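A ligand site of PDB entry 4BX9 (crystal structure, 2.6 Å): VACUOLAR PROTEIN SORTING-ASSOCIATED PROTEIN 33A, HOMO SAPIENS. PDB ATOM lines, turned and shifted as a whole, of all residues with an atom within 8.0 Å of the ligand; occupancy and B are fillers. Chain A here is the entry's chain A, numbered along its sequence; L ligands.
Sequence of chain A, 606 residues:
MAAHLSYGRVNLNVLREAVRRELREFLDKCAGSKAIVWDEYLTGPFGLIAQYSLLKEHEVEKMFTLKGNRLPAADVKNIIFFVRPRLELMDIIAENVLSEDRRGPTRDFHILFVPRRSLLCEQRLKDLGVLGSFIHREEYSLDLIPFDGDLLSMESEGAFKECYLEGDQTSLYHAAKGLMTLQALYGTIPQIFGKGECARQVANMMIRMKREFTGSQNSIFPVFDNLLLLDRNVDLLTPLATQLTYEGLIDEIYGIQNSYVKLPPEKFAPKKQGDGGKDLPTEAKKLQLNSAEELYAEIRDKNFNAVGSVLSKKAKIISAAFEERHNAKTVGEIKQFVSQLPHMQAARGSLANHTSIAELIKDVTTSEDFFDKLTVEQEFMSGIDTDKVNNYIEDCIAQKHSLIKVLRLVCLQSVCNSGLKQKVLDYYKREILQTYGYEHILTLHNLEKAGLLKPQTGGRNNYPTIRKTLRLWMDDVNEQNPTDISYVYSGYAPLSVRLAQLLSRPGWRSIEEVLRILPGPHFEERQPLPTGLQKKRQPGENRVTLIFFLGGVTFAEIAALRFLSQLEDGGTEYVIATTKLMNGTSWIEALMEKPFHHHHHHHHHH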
ATOM      1  N   PRO A  85     -16.626 -23.581  33.678  1.00  0.00           N
ATOM      2  CA  PRO A  85     -16.580 -24.610  32.662  1.00  0.00           C
ATOM      3  C   PRO A  85     -15.939 -25.831  33.279  1.00  0.00           C
ATOM      4  O   PRO A  85     -14.761 -26.133  33.019  1.00  0.00           O
ATOM      5  CB  PRO A  85     -15.668 -24.013  31.581  1.00  0.00           C
ATOM      6  CG  PRO A  85     -14.790 -23.021  32.288  1.00  0.00           C
ATOM      7  CD  PRO A  85     -15.595 -22.545  33.460  1.00  0.00           C
ATOM      8  N   ARG A 116     -14.980 -18.632  31.045  1.00  0.00           N
ATOM      9  CA  ARG A 116     -14.861 -18.978  29.607  1.00  0.00           C
ATOM     10  C   ARG A 116     -15.821 -20.057  29.248  1.00  0.00           C
ATOM     11  O   ARG A 116     -16.066 -20.931  30.067  1.00  0.00           O
ATOM     12  CB  ARG A 116     -13.462 -19.522  29.367  1.00  0.00           C
ATOM     13  CG  ARG A 116     -13.055 -19.650  27.934  1.00  0.00           C
ATOM     14  CD  ARG A 116     -11.640 -20.265  27.838  1.00  0.00           C
ATOM     15  NE  ARG A 116     -11.528 -21.587  28.481  1.00  0.00           N
ATOM     16  CZ  ARG A 116     -11.810 -22.757  27.899  1.00  0.00           C
ATOM     17  NH1 ARG A 116     -12.256 -22.821  26.653  1.00  0.00           N
ATOM     18  NH2 ARG A 116     -11.671 -23.867  28.603  1.00  0.00           N
ATOM     19  N   ARG A 117     -16.380 -20.042  28.036  1.00  0.00           N
ATOM     20  CA  ARG A 117     -17.124 -21.221  27.585  1.00  0.00           C
ATOM     21  C   ARG A 117     -16.253 -22.280  26.939  1.00  0.00           C
ATOM     22  O   ARG A 117     -15.246 -21.957  26.385  1.00  0.00           O
ATOM     23  CB  ARG A 117     -18.303 -20.847  26.720  1.00  0.00           C
ATOM     24  CG  ARG A 117     -17.948 -20.393  25.346  1.00  0.00           C
ATOM     25  CD  ARG A 117     -19.067 -19.516  24.791  1.00  0.00           C
ATOM     26  NE  ARG A 117     -20.187 -20.304  24.322  1.00  0.00           N
ATOM     27  CZ  ARG A 117     -20.223 -20.912  23.151  1.00  0.00           C
ATOM     28  NH1 ARG A 117     -19.192 -20.863  22.334  1.00  0.00           N
ATOM     29  NH2 ARG A 117     -21.292 -21.608  22.803  1.00  0.00           N
ATOM     30  N   SER A 118     -16.631 -23.549  27.078  1.00  0.00           N
ATOM     31  CA  SER A 118     -15.751 -24.641  26.778  1.00  0.00           C
ATOM     32  C   SER A 118     -16.446 -25.510  25.777  1.00  0.00           C
ATOM     33  O   SER A 118     -17.551 -25.921  26.030  1.00  0.00           O
ATOM     34  CB  SER A 118     -15.494 -25.451  28.050  1.00  0.00           C
ATOM     35  OG  SER A 118     -14.873 -26.718  27.765  1.00  0.00           O
ATOM     36  N   LEU A 119     -15.811 -25.784  24.633  1.00  0.00           N
ATOM     37  CA  LEU A 119     -16.426 -26.666  23.620  1.00  0.00           C
ATOM     38  C   LEU A 119     -16.755 -28.033  24.211  1.00  0.00           C
ATOM     39  O   LEU A 119     -17.821 -28.609  24.006  1.00  0.00           O
ATOM     40  CB  LEU A 119     -15.586 -26.764  22.318  1.00  0.00           C
ATOM     41  CG  LEU A 119     -15.450 -25.418  21.515  1.00  0.00           C
ATOM     42  CD1 LEU A 119     -14.601 -25.585  20.264  1.00  0.00           C
ATOM     43  CD2 LEU A 119     -16.801 -24.769  21.155  1.00  0.00           C
ATOM     44  N   LEU A 120     -15.835 -28.509  25.017  1.00  0.00           N
ATOM     45  CA  LEU A 120     -15.969 -29.761  25.662  1.00  0.00           C
ATOM     46  C   LEU A 120     -17.194 -29.829  26.603  1.00  0.00           C
ATOM     47  O   LEU A 120     -17.876 -30.860  26.590  1.00  0.00           O
ATOM     48  CB  LEU A 120     -14.691 -30.025  26.428  1.00  0.00           C
ATOM     49  CG  LEU A 120     -14.840 -31.324  27.200  1.00  0.00           C
ATOM     50  CD1 LEU A 120     -15.103 -32.499  26.244  1.00  0.00           C
ATOM     51  CD2 LEU A 120     -13.584 -31.504  28.024  1.00  0.00           C
ATOM     52  N   CYS A 121     -17.416 -28.795  27.442  1.00  0.00           N
ATOM     53  CA  CYS A 121     -18.580 -28.774  28.325  1.00  0.00           C
ATOM     54  C   CYS A 121     -19.896 -28.762  27.561  1.00  0.00           C
ATOM     55  O   CYS A 121     -20.856 -29.451  27.935  1.00  0.00           O
ATOM     56  CB  CYS A 121     -18.560 -27.572  29.243  1.00  0.00           C
ATOM     57  SG  CYS A 121     -17.332 -27.787  30.569  1.00  0.00           S
ATOM     58  N   GLU A 122     -19.912 -28.036  26.467  1.00  0.00           N
ATOM     59  CA  GLU A 122     -21.083 -28.003  25.600  1.00  0.00           C
ATOM     60  C   GLU A 122     -21.336 -29.378  24.987  1.00  0.00           C
ATOM     61  O   GLU A 122     -22.477 -29.837  24.907  1.00  0.00           O
ATOM     62  CB  GLU A 122     -20.962 -26.857  24.601  1.00  0.00           C
ATOM     63  CG  GLU A 122     -21.313 -25.495  25.292  1.00  0.00           C
ATOM     64  CD  GLU A 122     -21.183 -24.261  24.404  1.00  0.00           C
ATOM     65  OE1 GLU A 122     -20.791 -24.369  23.203  1.00  0.00           O
ATOM     66  OE2 GLU A 122     -21.455 -23.149  24.926  1.00  0.00           O
ATOM     67  N   GLN A 123     -20.246 -30.075  24.635  1.00  0.00           N
ATOM     68  CA  GLN A 123     -20.370 -31.424  24.057  1.00  0.00           C
ATOM     69  C   GLN A 123     -21.020 -32.347  25.097  1.00  0.00           C
ATOM     70  O   GLN A 123     -21.843 -33.228  24.755  1.00  0.00           O
ATOM     71  CB  GLN A 123     -19.016 -31.978  23.609  1.00  0.00           C
ATOM     72  CG  GLN A 123     -19.125 -33.411  23.130  1.00  0.00           C
ATOM     73  CD  GLN A 123     -19.826 -33.531  21.792  1.00  0.00           C
ATOM     74  OE1 GLN A 123     -19.652 -32.679  20.931  1.00  0.00           O
ATOM     75  NE2 GLN A 123     -20.619 -34.582  21.614  1.00  0.00           N
ATOM     76  N   GLU A 139     -20.373 -16.475  27.388  1.00  0.00           N
ATOM     77  CA  GLU A 139     -19.323 -16.392  28.392  1.00  0.00           C
ATOM     78  C   GLU A 139     -19.219 -14.976  28.963  1.00  0.00           C
ATOM     79  O   GLU A 139     -19.518 -14.033  28.276  1.00  0.00           O
ATOM     80  CB  GLU A 139     -18.000 -16.838  27.797  1.00  0.00           C
ATOM     81  CG  GLU A 139     -17.351 -15.897  26.822  1.00  0.00           C
ATOM     82  CD  GLU A 139     -16.157 -16.539  26.089  1.00  0.00           C
ATOM     83  OE1 GLU A 139     -15.629 -17.612  26.544  1.00  0.00           O
ATOM     84  OE2 GLU A 139     -15.739 -15.968  25.042  1.00  0.00           O
ATOM     85  N   TYR A 173      -2.922 -18.524  31.134  1.00  0.00           N
ATOM     86  CA  TYR A 173      -3.741 -18.104  30.025  1.00  0.00           C
ATOM     87  C   TYR A 173      -4.740 -17.013  30.483  1.00  0.00           C
ATOM     88  O   TYR A 173      -4.902 -16.011  29.833  1.00  0.00           O
ATOM     89  CB  TYR A 173      -4.454 -19.303  29.376  1.00  0.00           C
ATOM     90  CG  TYR A 173      -5.509 -18.920  28.352  1.00  0.00           C
ATOM     91  CD1 TYR A 173      -5.213 -18.711  27.027  1.00  0.00           C
ATOM     92  CD2 TYR A 173      -6.831 -18.739  28.765  1.00  0.00           C
ATOM     93  CE1 TYR A 173      -6.208 -18.346  26.108  1.00  0.00           C
ATOM     94  CE2 TYR A 173      -7.831 -18.369  27.891  1.00  0.00           C
ATOM     95  CZ  TYR A 173      -7.525 -18.156  26.557  1.00  0.00           C
ATOM     96  OH  TYR A 173      -8.550 -17.791  25.671  1.00  0.00           O
HETATM   97  C1  LIG L   1     -12.311 -26.913  25.946  1.00  0.00           C
HETATM   98  O1  LIG L   1     -12.335 -27.319  27.159  1.00  0.00           O
HETATM   99  O2  LIG L   1     -13.261 -27.119  25.135  1.00  0.00           O
HETATM  100  C2  LIG L   1     -11.089 -26.156  25.449  1.00  0.00           C
HETATM  101  O3  LIG L   1      -9.939 -26.938  25.799  1.00  0.00           O
HETATM  102  C3  LIG L   1     -11.123 -25.909  23.919  1.00  0.00           C
HETATM  103  C4  LIG L   1     -12.066 -24.714  23.619  1.00  0.00           C
HETATM  104  O4  LIG L   1     -11.629 -23.812  22.870  1.00  0.00           O
HETATM  105  O5  LIG L   1     -13.249 -24.602  24.145  1.00  0.00           O
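The side-chain hydroxyl (OG) of Ser 118 sits close to the backbone NH (N) of Leu 120, 3.4 Å away. N of Cys 121 sits at hydrogen-bond distance from OG of Ser 118 (3.3 Å). The side-chain carboxylate (OE2) of Glu 122 lies within salt-bridge range of the guanidinium group (NH2) of Arg 117, at 2.6 Å. The backbone NH (N) of Arg 117 lies within hydrogen-bond range of the side-chain carboxylate (OE1) of Glu 139, at 2.9 Å.
Hydrophobic or aromatic side chains within 4 Å of the ligand: Leu 119 and Leu 120.
The side-chain hydroxyl (OG) of Ser 118 sits at hydrogen-bond distance from an oxygen (O1) of the ligand (2.7 Å). The backbone NH (N) of Leu 119 lies within hydrogen-bond range of an oxygen (O5) of the ligand, 2.9 Å away. N of Leu 120 sits at hydrogen-bond distance from O2 of the ligand (2.9 Å). The guanidinium group of Arg 116 lies within salt-bridge range of an oxygen (O5) of the ligand, at 3.2 Å.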
